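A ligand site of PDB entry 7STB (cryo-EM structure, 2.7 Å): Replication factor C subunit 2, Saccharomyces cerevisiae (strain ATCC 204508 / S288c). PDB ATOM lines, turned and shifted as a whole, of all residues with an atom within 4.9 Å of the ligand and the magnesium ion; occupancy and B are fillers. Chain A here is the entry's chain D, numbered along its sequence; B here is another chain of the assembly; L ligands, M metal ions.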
ATOM      1  N   TRP A  27     -16.029  -2.014 -38.880  1.00  0.00           N
ATOM      2  CA  TRP A  27     -17.167  -2.931 -38.924  1.00  0.00           C
ATOM      3  C   TRP A  27     -18.092  -2.721 -37.739  1.00  0.00           C
ATOM      4  O   TRP A  27     -19.318  -2.822 -37.867  1.00  0.00           O
ATOM      5  CB  TRP A  27     -16.670  -4.375 -38.965  1.00  0.00           C
ATOM      6  CG  TRP A  27     -16.060  -4.758 -40.280  1.00  0.00           C
ATOM      7  CD1 TRP A  27     -15.622  -3.917 -41.258  1.00  0.00           C
ATOM      8  CD2 TRP A  27     -15.812  -6.086 -40.757  1.00  0.00           C
ATOM      9  NE1 TRP A  27     -15.123  -4.635 -42.314  1.00  0.00           N
ATOM     10  CE2 TRP A  27     -15.225  -5.965 -42.027  1.00  0.00           C
ATOM     11  CE3 TRP A  27     -16.021  -7.364 -40.228  1.00  0.00           C
ATOM     12  CZ2 TRP A  27     -14.855  -7.074 -42.780  1.00  0.00           C
ATOM     13  CZ3 TRP A  27     -15.652  -8.466 -40.974  1.00  0.00           C
ATOM     14  CH2 TRP A  27     -15.075  -8.311 -42.240  1.00  0.00           C
ATOM     15  N   VAL A  28     -17.530  -2.431 -36.562  1.00  0.00           N
ATOM     16  CA  VAL A  28     -18.370  -2.195 -35.390  1.00  0.00           C
ATOM     17  C   VAL A  28     -19.252  -0.962 -35.603  1.00  0.00           C
ATOM     18  O   VAL A  28     -20.445  -0.979 -35.264  1.00  0.00           O
ATOM     19  CB  VAL A  28     -17.496  -2.044 -34.125  1.00  0.00           C
ATOM     20  CG1 VAL A  28     -16.805  -3.360 -33.808  1.00  0.00           C
ATOM     21  CG2 VAL A  28     -16.476  -0.913 -34.278  1.00  0.00           C
ATOM     22  N   TYR A  31     -22.002  -1.597 -38.533  1.00  0.00           N
ATOM     23  CA  TYR A  31     -23.070  -2.547 -38.244  1.00  0.00           C
ATOM     24  C   TYR A  31     -23.800  -2.227 -36.944  1.00  0.00           C
ATOM     25  O   TYR A  31     -24.405  -3.114 -36.336  1.00  0.00           O
ATOM     26  CB  TYR A  31     -22.510  -3.971 -38.187  1.00  0.00           C
ATOM     27  CG  TYR A  31     -22.130  -4.520 -39.542  1.00  0.00           C
ATOM     28  CD1 TYR A  31     -20.874  -4.298 -40.091  1.00  0.00           C
ATOM     29  CD2 TYR A  31     -23.049  -5.257 -40.291  1.00  0.00           C
ATOM     30  CE1 TYR A  31     -20.533  -4.798 -41.326  1.00  0.00           C
ATOM     31  CE2 TYR A  31     -22.718  -5.760 -41.525  1.00  0.00           C
ATOM     32  CZ  TYR A  31     -21.459  -5.534 -42.045  1.00  0.00           C
ATOM     33  OH  TYR A  31     -21.127  -6.037 -43.279  1.00  0.00           O
ATOM     34  N   ARG A  32     -23.756  -0.971 -36.506  1.00  0.00           N
ATOM     35  CA  ARG A  32     -24.475  -0.596 -35.299  1.00  0.00           C
ATOM     36  C   ARG A  32     -25.980  -0.736 -35.534  1.00  0.00           C
ATOM     37  O   ARG A  32     -26.500  -0.183 -36.505  1.00  0.00           O
ATOM     38  CB  ARG A  32     -24.134   0.843 -34.902  1.00  0.00           C
ATOM     39  CG  ARG A  32     -24.920   1.360 -33.704  1.00  0.00           C
ATOM     40  CD  ARG A  32     -24.451   2.737 -33.286  1.00  0.00           C
ATOM     41  NE  ARG A  32     -23.050   2.745 -32.888  1.00  0.00           N
ATOM     42  CZ  ARG A  32     -22.606   2.409 -31.690  1.00  0.00           C
ATOM     43  NH1 ARG A  32     -23.421   2.027 -30.722  1.00  0.00           N
ATOM     44  NH2 ARG A  32     -21.293   2.459 -31.437  1.00  0.00           N
ATOM     45  N   PRO A  33     -26.700  -1.477 -34.686  1.00  0.00           N
ATOM     46  CA  PRO A  33     -28.153  -1.589 -34.865  1.00  0.00           C
ATOM     47  C   PRO A  33     -28.809  -0.239 -35.089  1.00  0.00           C
ATOM     48  O   PRO A  33     -28.598   0.709 -34.320  1.00  0.00           O
ATOM     49  CB  PRO A  33     -28.611  -2.239 -33.556  1.00  0.00           C
ATOM     50  CG  PRO A  33     -27.399  -2.936 -32.998  1.00  0.00           C
ATOM     51  CD  PRO A  33     -26.185  -2.522 -33.779  1.00  0.00           C
ATOM     52  N   GLU A  38     -33.241  -5.521 -34.705  1.00  0.00           N
ATOM     53  CA  GLU A  38     -32.007  -6.246 -34.978  1.00  0.00           C
ATOM     54  C   GLU A  38     -31.099  -6.372 -33.770  1.00  0.00           C
ATOM     55  O   GLU A  38     -29.954  -6.816 -33.907  1.00  0.00           O
ATOM     56  CB  GLU A  38     -31.254  -5.594 -36.149  1.00  0.00           C
ATOM     57  CG  GLU A  38     -30.919  -4.128 -35.940  1.00  0.00           C
ATOM     58  CD  GLU A  38     -30.462  -3.461 -37.223  1.00  0.00           C
ATOM     59  OE1 GLU A  38     -30.369  -4.160 -38.263  1.00  0.00           O
ATOM     60  OE2 GLU A  38     -30.193  -2.246 -37.200  1.00  0.00           O
ATOM     61  N   VAL A  39     -31.568  -5.991 -32.579  1.00  0.00           N
ATOM     62  CA  VAL A  39     -30.821  -6.272 -31.364  1.00  0.00           C
ATOM     63  C   VAL A  39     -30.912  -7.769 -31.066  1.00  0.00           C
ATOM     64  O   VAL A  39     -32.004  -8.356 -31.096  1.00  0.00           O
ATOM     65  CB  VAL A  39     -31.351  -5.435 -30.189  1.00  0.00           C
ATOM     66  CG1 VAL A  39     -30.639  -5.804 -28.895  1.00  0.00           C
ATOM     67  CG2 VAL A  39     -31.172  -3.947 -30.488  1.00  0.00           C
ATOM     68  N   THR A  40     -29.769  -8.383 -30.789  1.00  0.00           N
ATOM     69  CA  THR A  40     -29.685  -9.838 -30.861  1.00  0.00           C
ATOM     70  C   THR A  40     -30.156 -10.523 -29.575  1.00  0.00           C
ATOM     71  O   THR A  40     -31.080 -11.339 -29.597  1.00  0.00           O
ATOM     72  CB  THR A  40     -28.257 -10.274 -31.210  1.00  0.00           C
ATOM     73  OG1 THR A  40     -28.204 -11.699 -31.353  1.00  0.00           O
ATOM     74  CG2 THR A  40     -27.246  -9.848 -30.142  1.00  0.00           C
ATOM     75  N   ALA A  41     -29.549 -10.193 -28.436  1.00  0.00           N
ATOM     76  CA  ALA A  41     -29.690 -10.986 -27.218  1.00  0.00           C
ATOM     77  C   ALA A  41     -30.071 -10.107 -26.029  1.00  0.00           C
ATOM     78  O   ALA A  41     -29.498 -10.202 -24.945  1.00  0.00           O
ATOM     79  CB  ALA A  41     -28.410 -11.755 -26.917  1.00  0.00           C
ATOM     80  N   GLN A  42     -31.054  -9.226 -26.226  1.00  0.00           N
ATOM     81  CA  GLN A  42     -31.590  -8.413 -25.148  1.00  0.00           C
ATOM     82  C   GLN A  42     -33.111  -8.390 -25.221  1.00  0.00           C
ATOM     83  O   GLN A  42     -33.750  -7.358 -25.008  1.00  0.00           O
ATOM     84  CB  GLN A  42     -31.023  -6.996 -25.190  1.00  0.00           C
ATOM     85  CG  GLN A  42     -29.518  -6.923 -25.449  1.00  0.00           C
ATOM     86  CD  GLN A  42     -28.697  -7.477 -24.304  1.00  0.00           C
ATOM     87  OE1 GLN A  42     -29.239  -8.072 -23.371  1.00  0.00           O
ATOM     88  NE2 GLN A  42     -27.386  -7.304 -24.380  1.00  0.00           N
ATOM     89  N   GLY A  65     -24.632  -3.064 -17.590  1.00  0.00           N
ATOM     90  CA  GLY A  65     -24.058  -4.276 -18.118  1.00  0.00           C
ATOM     91  C   GLY A  65     -22.588  -4.149 -18.494  1.00  0.00           C
ATOM     92  O   GLY A  65     -22.023  -3.059 -18.526  1.00  0.00           O
ATOM     93  N   PRO A  66     -21.953  -5.271 -18.788  1.00  0.00           N
ATOM     94  CA  PRO A  66     -20.524  -5.266 -19.124  1.00  0.00           C
ATOM     95  C   PRO A  66     -20.278  -4.598 -20.468  1.00  0.00           C
ATOM     96  O   PRO A  66     -21.228  -4.324 -21.222  1.00  0.00           O
ATOM     97  CB  PRO A  66     -20.150  -6.751 -19.160  1.00  0.00           C
ATOM     98  CG  PRO A  66     -21.428  -7.471 -19.368  1.00  0.00           C
ATOM     99  CD  PRO A  66     -22.502  -6.645 -18.746  1.00  0.00           C
ATOM    100  N   PRO A  67     -19.018  -4.321 -20.802  1.00  0.00           N
ATOM    101  CA  PRO A  67     -18.731  -3.555 -22.019  1.00  0.00           C
ATOM    102  C   PRO A  67     -19.225  -4.239 -23.280  1.00  0.00           C
ATOM    103  O   PRO A  67     -19.209  -5.465 -23.399  1.00  0.00           O
ATOM    104  CB  PRO A  67     -17.200  -3.439 -22.013  1.00  0.00           C
ATOM    105  CG  PRO A  67     -16.792  -3.696 -20.605  1.00  0.00           C
ATOM    106  CD  PRO A  67     -17.794  -4.664 -20.064  1.00  0.00           C
ATOM    107  N   GLY A  68     -19.657  -3.417 -24.235  1.00  0.00           N
ATOM    108  CA  GLY A  68     -20.036  -3.918 -25.545  1.00  0.00           C
ATOM    109  C   GLY A  68     -21.190  -4.895 -25.538  1.00  0.00           C
ATOM    110  O   GLY A  68     -21.140  -5.903 -26.244  1.00  0.00           O
ATOM    111  N   THR A  69     -22.227  -4.618 -24.749  1.00  0.00           N
ATOM    112  CA  THR A  69     -23.402  -5.471 -24.689  1.00  0.00           C
ATOM    113  C   THR A  69     -24.584  -4.909 -25.471  1.00  0.00           C
ATOM    114  O   THR A  69     -25.628  -5.566 -25.548  1.00  0.00           O
ATOM    115  CB  THR A  69     -23.821  -5.702 -23.239  1.00  0.00           C
ATOM    116  OG1 THR A  69     -23.748  -4.466 -22.508  1.00  0.00           O
ATOM    117  CG2 THR A  69     -22.914  -6.728 -22.579  1.00  0.00           C
ATOM    118  N   GLY A  70     -24.449  -3.726 -26.059  1.00  0.00           N
ATOM    119  CA  GLY A  70     -25.494  -3.145 -26.881  1.00  0.00           C
ATOM    120  C   GLY A  70     -26.409  -2.218 -26.109  1.00  0.00           C
ATOM    121  O   GLY A  70     -27.632  -2.277 -26.271  1.00  0.00           O
ATOM    122  N   LYS A  71     -25.829  -1.340 -25.288  1.00  0.00           N
ATOM    123  CA  LYS A  71     -26.622  -0.417 -24.487  1.00  0.00           C
ATOM    124  C   LYS A  71     -26.847   0.908 -25.209  1.00  0.00           C
ATOM    125  O   LYS A  71     -27.981   1.357 -25.339  1.00  0.00           O
ATOM    126  CB  LYS A  71     -25.934  -0.178 -23.146  1.00  0.00           C
ATOM    127  CG  LYS A  71     -25.721  -1.446 -22.323  1.00  0.00           C
ATOM    128  CD  LYS A  71     -25.265  -1.143 -20.905  1.00  0.00           C
ATOM    129  CE  LYS A  71     -23.810  -0.698 -20.865  1.00  0.00           C
ATOM    130  NZ  LYS A  71     -22.867  -1.793 -21.233  1.00  0.00           N
ATOM    131  N   THR A  72     -25.772   1.539 -25.684  1.00  0.00           N
ATOM    132  CA  THR A  72     -25.915   2.791 -26.427  1.00  0.00           C
ATOM    133  C   THR A  72     -26.696   2.572 -27.717  1.00  0.00           C
ATOM    134  O   THR A  72     -27.548   3.392 -28.094  1.00  0.00           O
ATOM    135  CB  THR A  72     -24.548   3.390 -26.724  1.00  0.00           C
ATOM    136  OG1 THR A  72     -23.826   3.563 -25.501  1.00  0.00           O
ATOM    137  CG2 THR A  72     -24.683   4.738 -27.423  1.00  0.00           C
ATOM    138  N   SER A  73     -26.414   1.468 -28.417  1.00  0.00           N
ATOM    139  CA  SER A  73     -27.133   1.175 -29.655  1.00  0.00           C
ATOM    140  C   SER A  73     -28.619   1.042 -29.399  1.00  0.00           C
ATOM    141  O   SER A  73     -29.441   1.535 -30.178  1.00  0.00           O
ATOM    142  CB  SER A  73     -26.568  -0.092 -30.290  1.00  0.00           C
ATOM    143  OG  SER A  73     -25.181   0.025 -30.534  1.00  0.00           O
ATOM    144  N   ASP A 140     -25.285   8.762 -20.740  1.00  0.00           N
ATOM    145  CA  ASP A 140     -24.431   7.612 -20.970  1.00  0.00           C
ATOM    146  C   ASP A 140     -23.232   7.649 -20.029  1.00  0.00           C
ATOM    147  O   ASP A 140     -22.700   8.712 -19.697  1.00  0.00           O
ATOM    148  CB  ASP A 140     -23.958   7.570 -22.416  1.00  0.00           C
ATOM    149  CG  ASP A 140     -23.824   6.170 -22.958  1.00  0.00           C
ATOM    150  OD1 ASP A 140     -23.532   5.246 -22.161  1.00  0.00           O
ATOM    151  OD2 ASP A 140     -23.999   5.973 -24.176  1.00  0.00           O
ATOM    152  N   GLU A 141     -22.805   6.458 -19.590  1.00  0.00           N
ATOM    153  CA  GLU A 141     -21.645   6.312 -18.724  1.00  0.00           C
ATOM    154  C   GLU A 141     -21.863   7.068 -17.404  1.00  0.00           C
ATOM    155  O   GLU A 141     -20.994   7.776 -16.911  1.00  0.00           O
ATOM    156  CB  GLU A 141     -20.380   6.802 -19.427  1.00  0.00           C
ATOM    157  CG  GLU A 141     -19.792   5.805 -20.404  1.00  0.00           C
ATOM    158  CD  GLU A 141     -19.165   6.473 -21.605  1.00  0.00           C
ATOM    159  OE1 GLU A 141     -18.449   7.487 -21.424  1.00  0.00           O
ATOM    160  OE2 GLU A 141     -19.389   5.999 -22.743  1.00  0.00           O
ATOM    161  N   ASN A 171     -21.749   0.471 -16.550  1.00  0.00           N
ATOM    162  CA  ASN A 171     -21.156  -0.854 -16.415  1.00  0.00           C
ATOM    163  C   ASN A 171     -21.117  -1.332 -14.967  1.00  0.00           C
ATOM    164  O   ASN A 171     -21.170  -2.538 -14.722  1.00  0.00           O
ATOM    165  CB  ASN A 171     -19.736  -0.864 -16.984  1.00  0.00           C
ATOM    166  CG  ASN A 171     -19.675  -0.398 -18.428  1.00  0.00           C
ATOM    167  OD1 ASN A 171     -19.356   0.758 -18.697  1.00  0.00           O
ATOM    168  ND2 ASN A 171     -19.990  -1.287 -19.349  1.00  0.00           N
ATOM    169  N   LEU A 192     -22.871 -11.537 -24.115  1.00  0.00           N
ATOM    170  CA  LEU A 192     -23.138 -12.178 -25.393  1.00  0.00           C
ATOM    171  C   LEU A 192     -22.085 -13.237 -25.657  1.00  0.00           C
ATOM    172  O   LEU A 192     -20.885 -12.934 -25.707  1.00  0.00           O
ATOM    173  CB  LEU A 192     -23.153 -11.146 -26.520  1.00  0.00           C
ATOM    174  CG  LEU A 192     -24.232 -10.069 -26.392  1.00  0.00           C
ATOM    175  CD1 LEU A 192     -23.635  -8.796 -25.826  1.00  0.00           C
ATOM    176  CD2 LEU A 192     -24.899  -9.793 -27.723  1.00  0.00           C
ATOM    177  N   ARG A 200     -25.761 -12.905 -35.068  1.00  0.00           N
ATOM    178  CA  ARG A 200     -25.368 -11.577 -35.538  1.00  0.00           C
ATOM    179  C   ARG A 200     -23.974 -11.600 -36.174  1.00  0.00           C
ATOM    180  O   ARG A 200     -23.763 -10.988 -37.229  1.00  0.00           O
ATOM    181  CB  ARG A 200     -25.406 -10.589 -34.372  1.00  0.00           C
ATOM    182  CG  ARG A 200     -25.074  -9.154 -34.747  1.00  0.00           C
ATOM    183  CD  ARG A 200     -26.027  -8.614 -35.811  1.00  0.00           C
ATOM    184  NE  ARG A 200     -25.821  -7.196 -36.069  1.00  0.00           N
ATOM    185  CZ  ARG A 200     -26.432  -6.507 -37.017  1.00  0.00           C
ATOM    186  NH1 ARG A 200     -27.308  -7.070 -37.819  1.00  0.00           N
ATOM    187  NH2 ARG A 200     -26.160  -5.207 -37.155  1.00  0.00           N
ATOM    188  N   LEU A 228     -19.496  -8.377 -27.909  1.00  0.00           N
ATOM    189  CA  LEU A 228     -19.632  -8.534 -29.351  1.00  0.00           C
ATOM    190  C   LEU A 228     -18.764  -7.545 -30.116  1.00  0.00           C
ATOM    191  O   LEU A 228     -18.373  -7.821 -31.260  1.00  0.00           O
ATOM    192  CB  LEU A 228     -21.099  -8.371 -29.761  1.00  0.00           C
ATOM    193  CG  LEU A 228     -21.492  -8.926 -31.135  1.00  0.00           C
ATOM    194  CD1 LEU A 228     -21.066 -10.374 -31.311  1.00  0.00           C
ATOM    195  CD2 LEU A 228     -22.994  -8.788 -31.338  1.00  0.00           C
ATOM    196  N   ARG A 229     -18.439  -6.402 -29.518  1.00  0.00           N
ATOM    197  CA  ARG A 229     -17.553  -5.450 -30.173  1.00  0.00           C
ATOM    198  C   ARG A 229     -16.181  -6.060 -30.410  1.00  0.00           C
ATOM    199  O   ARG A 229     -15.601  -5.935 -31.500  1.00  0.00           O
ATOM    200  CB  ARG A 229     -17.436  -4.169 -29.331  1.00  0.00           C
ATOM    201  CG  ARG A 229     -16.907  -2.976 -30.094  1.00  0.00           C
ATOM    202  CD  ARG A 229     -16.255  -1.949 -29.184  1.00  0.00           C
ATOM    203  NE  ARG A 229     -17.216  -0.969 -28.686  1.00  0.00           N
ATOM    204  CZ  ARG A 229     -17.779  -0.998 -27.486  1.00  0.00           C
ATOM    205  NH1 ARG A 229     -17.528  -1.960 -26.623  1.00  0.00           N
ATOM    206  NH2 ARG A 229     -18.615  -0.020 -27.145  1.00  0.00           N
ATOM    207  N   ILE A 232     -16.411  -8.614 -33.234  1.00  0.00           N
ATOM    208  CA  ILE A 232     -16.496  -7.992 -34.550  1.00  0.00           C
ATOM    209  C   ILE A 232     -15.131  -7.448 -34.969  1.00  0.00           C
ATOM    210  O   ILE A 232     -14.720  -7.591 -36.124  1.00  0.00           O
ATOM    211  CB  ILE A 232     -17.570  -6.894 -34.553  1.00  0.00           C
ATOM    212  CG1 ILE A 232     -18.953  -7.511 -34.332  1.00  0.00           C
ATOM    213  CG2 ILE A 232     -17.550  -6.133 -35.868  1.00  0.00           C
ATOM    214  CD1 ILE A 232     -19.958  -6.545 -33.733  1.00  0.00           C
ATOM    215  N   ARG B 155     -13.947   6.972 -24.651  1.00  0.00           N
ATOM    216  CA  ARG B 155     -14.820   5.957 -25.251  1.00  0.00           C
ATOM    217  C   ARG B 155     -15.717   6.551 -26.320  1.00  0.00           C
ATOM    218  O   ARG B 155     -15.624   6.191 -27.507  1.00  0.00           O
ATOM    219  CB  ARG B 155     -15.653   5.288 -24.155  1.00  0.00           C
ATOM    220  CG  ARG B 155     -14.846   4.566 -23.097  1.00  0.00           C
ATOM    221  CD  ARG B 155     -15.680   4.273 -21.864  1.00  0.00           C
ATOM    222  NE  ARG B 155     -16.937   3.632 -22.191  1.00  0.00           N
ATOM    223  CZ  ARG B 155     -17.789   3.127 -21.305  1.00  0.00           C
ATOM    224  NH1 ARG B 155     -17.535   3.176 -20.007  1.00  0.00           N
ATOM    225  NH2 ARG B 155     -18.915   2.565 -21.728  1.00  0.00           N
ATOM    226  N   ARG B 156     -16.610   7.463 -25.929  1.00  0.00           N
ATOM    227  CA  ARG B 156     -17.551   8.014 -26.895  1.00  0.00           C
ATOM    228  C   ARG B 156     -16.868   8.940 -27.889  1.00  0.00           C
ATOM    229  O   ARG B 156     -17.337   9.088 -29.013  1.00  0.00           O
ATOM    230  CB  ARG B 156     -18.680   8.756 -26.171  1.00  0.00           C
ATOM    231  CG  ARG B 156     -19.662   7.846 -25.446  1.00  0.00           C
ATOM    232  CD  ARG B 156     -20.471   6.986 -26.415  1.00  0.00           C
ATOM    233  NE  ARG B 156     -21.289   7.784 -27.316  1.00  0.00           N
ATOM    234  CZ  ARG B 156     -21.826   7.335 -28.442  1.00  0.00           C
ATOM    235  NH1 ARG B 156     -21.645   6.088 -28.842  1.00  0.00           N
ATOM    236  NH2 ARG B 156     -22.564   8.156 -29.183  1.00  0.00           N
ATOM    237  N   GLU B 159     -15.835   6.407 -30.438  1.00  0.00           N
ATOM    238  CA  GLU B 159     -16.964   5.766 -31.109  1.00  0.00           C
ATOM    239  C   GLU B 159     -17.687   6.718 -32.046  1.00  0.00           C
ATOM    240  O   GLU B 159     -18.057   6.347 -33.164  1.00  0.00           O
ATOM    241  CB  GLU B 159     -17.944   5.201 -30.072  1.00  0.00           C
ATOM    242  CG  GLU B 159     -17.586   3.812 -29.588  1.00  0.00           C
ATOM    243  CD  GLU B 159     -18.673   3.208 -28.714  1.00  0.00           C
ATOM    244  OE1 GLU B 159     -19.223   3.953 -27.870  1.00  0.00           O
ATOM    245  OE2 GLU B 159     -18.956   2.008 -28.866  1.00  0.00           O
ATOM    246  N   PRO B 180     -13.441  -0.987 -21.199  1.00  0.00           N
ATOM    247  CA  PRO B 180     -14.045  -0.374 -22.397  1.00  0.00           C
ATOM    248  C   PRO B 180     -13.031   0.005 -23.459  1.00  0.00           C
ATOM    249  O   PRO B 180     -13.302  -0.176 -24.654  1.00  0.00           O
ATOM    250  CB  PRO B 180     -14.765   0.853 -21.826  1.00  0.00           C
ATOM    251  CG  PRO B 180     -15.023   0.530 -20.405  1.00  0.00           C
ATOM    252  CD  PRO B 180     -13.850  -0.300 -19.964  1.00  0.00           C
ATOM    253  N   ARG B 184     -12.729  -1.276 -27.279  1.00  0.00           N
ATOM    254  CA  ARG B 184     -12.858  -0.355 -28.409  1.00  0.00           C
ATOM    255  C   ARG B 184     -11.637  -0.328 -29.311  1.00  0.00           C
ATOM    256  O   ARG B 184     -11.689   0.310 -30.374  1.00  0.00           O
ATOM    257  CB  ARG B 184     -13.137   1.056 -27.895  1.00  0.00           C
ATOM    258  CG  ARG B 184     -14.595   1.350 -27.619  1.00  0.00           C
ATOM    259  CD  ARG B 184     -14.773   2.595 -26.782  1.00  0.00           C
ATOM    260  NE  ARG B 184     -16.169   2.886 -26.520  1.00  0.00           N
ATOM    261  CZ  ARG B 184     -16.923   2.233 -25.642  1.00  0.00           C
ATOM    262  NH1 ARG B 184     -16.429   1.235 -24.918  1.00  0.00           N
ATOM    263  NH2 ARG B 184     -18.194   2.588 -25.473  1.00  0.00           N
HETATM  264  P1  LIG L   1     -20.133   0.012 -23.308  1.00  0.00           P
HETATM  265  S1  LIG L   1     -18.205  -0.140 -23.045  1.00  0.00           S
HETATM  266  O1  LIG L   1     -20.475   1.451 -23.786  1.00  0.00           O
HETATM  267  O2  LIG L   1     -20.860  -0.267 -21.960  1.00  0.00           O
HETATM  268  P2  LIG L   1     -21.975  -0.832 -25.135  1.00  0.00           P
HETATM  269  O3  LIG L   1     -23.011  -1.703 -24.544  1.00  0.00           O
HETATM  270  O4  LIG L   1     -22.320   0.659 -25.038  1.00  0.00           O
HETATM  271  O5  LIG L   1     -20.596  -1.019 -24.375  1.00  0.00           O
HETATM  272  P3  LIG L   1     -22.433  -0.234 -27.788  1.00  0.00           P
HETATM  273  O6  LIG L   1     -23.879  -0.520 -27.933  1.00  0.00           O
HETATM  274  O7  LIG L   1     -22.117   1.210 -27.403  1.00  0.00           O
HETATM  275  O8  LIG L   1     -21.778  -1.157 -26.682  1.00  0.00           O
HETATM  276  O9  LIG L   1     -21.729  -0.633 -29.140  1.00  0.00           O
HETATM  277  C1  LIG L   1     -20.959  -1.840 -29.275  1.00  0.00           C
HETATM  278  C2  LIG L   1     -21.019  -2.307 -30.712  1.00  0.00           C
HETATM  279  O10 LIG L   1     -21.030  -3.745 -30.746  1.00  0.00           O
HETATM  280  C3  LIG L   1     -22.249  -1.857 -31.483  1.00  0.00           C
HETATM  281  O11 LIG L   1     -22.003  -0.639 -32.181  1.00  0.00           O
HETATM  282  C4  LIG L   1     -22.503  -3.027 -32.437  1.00  0.00           C
HETATM  283  O12 LIG L   1     -21.698  -2.948 -33.612  1.00  0.00           O
HETATM  284  C5  LIG L   1     -22.088  -4.212 -31.574  1.00  0.00           C
HETATM  285  N1  LIG L   1     -23.142  -4.724 -30.707  1.00  0.00           N
HETATM  286  C6  LIG L   1     -23.182  -4.682 -29.339  1.00  0.00           C
HETATM  287  N2  LIG L   1     -24.271  -5.218 -28.823  1.00  0.00           N
HETATM  288  C7  LIG L   1     -24.996  -5.629 -29.925  1.00  0.00           C
HETATM  289  C8  LIG L   1     -26.248  -6.261 -30.061  1.00  0.00           C
HETATM  290  N3  LIG L   1     -27.008  -6.613 -29.023  1.00  0.00           N
HETATM  291  N4  LIG L   1     -26.680  -6.529 -31.313  1.00  0.00           N
HETATM  292  C9  LIG L   1     -25.919  -6.177 -32.350  1.00  0.00           C
HETATM  293  N5  LIG L   1     -24.731  -5.576 -32.347  1.00  0.00           N
HETATM  294  C10 LIG L   1     -24.316  -5.321 -31.099  1.00  0.00           C
HETATM  295 MG    MG M   1     -21.656   3.156 -24.442  1.00  0.00          MG
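The backbone carbonyl oxygen of Val 28 lies within hydrogen-bond range of an oxygen (O12) of the ligand (2.9 Å). O6 of the ligand sits at hydrogen-bond distance from N of Ser 73 (3.3 Å). NH2 of Arg 229 is in salt-bridge range of O7 of the ligand (3.7 Å). The side-chain hydroxyl (OG) of Ser 73 sits at hydrogen-bond distance from an oxygen (O6) of the ligand, at 3.0 Å. The side-chain amino group of Lys 71 lies within salt-bridge range of an oxygen (O3) of the ligand. An oxygen (O3) of the ligand sits at hydrogen-bond distance from the backbone NH (N) of Lys 71, at 2.9 Å. The guanidinium group (NH2) of Arg 155 of chain B sits close to a sulfur (S1) of the ligand (3.1 Å). The backbone NH (N) of Gly 70 is in hydrogen-bond range of an oxygen (O3) of the ligand, at 2.9 Å. S1 of the ligand sits close to NH1 of Arg 184 of chain B. ND2 of Asn 171 sits at hydrogen-bond distance from O2 of the ligand. N of Thr 69 sits at hydrogen-bond distance from O3 of the ligand (3.0 Å). The guanidinium group of Arg 32 lies within salt-bridge range of an oxygen (O7) of the ligand, 3.7 Å away. The backbone NH (N) of Gly 68 sits at hydrogen-bond distance from an oxygen (O5) of the ligand (2.6 Å).
The side-chain carboxylate (OE2) of Glu 141 lies within salt-bridge range of the guanidinium group (NE) of Arg 155 of chain B (3.5 Å). OE2 of Glu 159 of chain B lies within salt-bridge range of NH2 of Arg 229 (2.7 Å). NH2 of Arg 32 lies within salt-bridge range of OE2 of Glu 159 of chain B, 3.5 Å away. NZ of Lys 71 lies within hydrogen-bond range of OG1 of Thr 69, at 3.1 Å. The side-chain hydroxyl (OG1) of Thr 69 sits at hydrogen-bond distance from the backbone carbonyl oxygen (O) of Pro 66 (2.8 Å). The backbone carbonyl oxygen of Gly 65 lies within hydrogen-bond range of the side-chain amide nitrogen of Asn 171 (2.8 Å). The backbone carbonyl oxygen (O) of Thr 69 sits at hydrogen-bond distance from the side-chain amide nitrogen (NE2) of Gln 42. OG of Ser 73 lies within hydrogen-bond range of NH1 of Arg 32, 2.7 Å away.
Merely in contact with the ligand: Tyr 31 (3.8 Å), Pro 33 (3.6 Å), Val 39 (3.7 Å), Thr 40 (3.4 Å), Pro 67 (3.6 Å), Arg 200 (3.9 Å), Leu 228 (3.7 Å), Ile 232 (3.8 Å), Glu 159 of chain B (3.6 Å) and Pro 180 of chain B (3.8 Å). Hydrophobic or aromatic side chains that line the ligand: Pro 33, Val 39, Pro 67, Leu 228, Ile 232 and Pro 180 of chain B. 22 residues have an atom within 4 Å of the ligand: Val 28, Tyr 31, Arg 32, Pro 33, Val 39, Thr 40, Pro 67, Gly 68, Thr 69, Gly 70, Lys 71, Thr 72, Ser 73, Asn 171, Arg 200, Leu 228, Arg 229, Ile 232, Arg 155 of chain B, Glu 159 of chain B, Pro 180 of chain B and Arg 184 of chain B.
Residues that only touch the magnesium ion: Asp 140 (3.6 Å), Arg 155 of chain B (3.9 Å) and Arg 184 of chain B (3.7 Å). Within 4 Å of the magnesium ion: Thr 72, Asp 140, Arg 155 of chain B and Arg 184 of chain B. The nearest printed residue that does not touch the magnesium ion is Glu 141 (4.01 Å).
The magnesium ion is bound by an oxygen (O1) of the ligand (2.2 Å) and the side-chain hydroxyl (OG1) of Thr 72 (2.4 Å). The magnesium ion has two donor atoms within binding distance. Slightly farther from the magnesium ion lies an oxygen (O4) of the ligand (2.7 Å).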
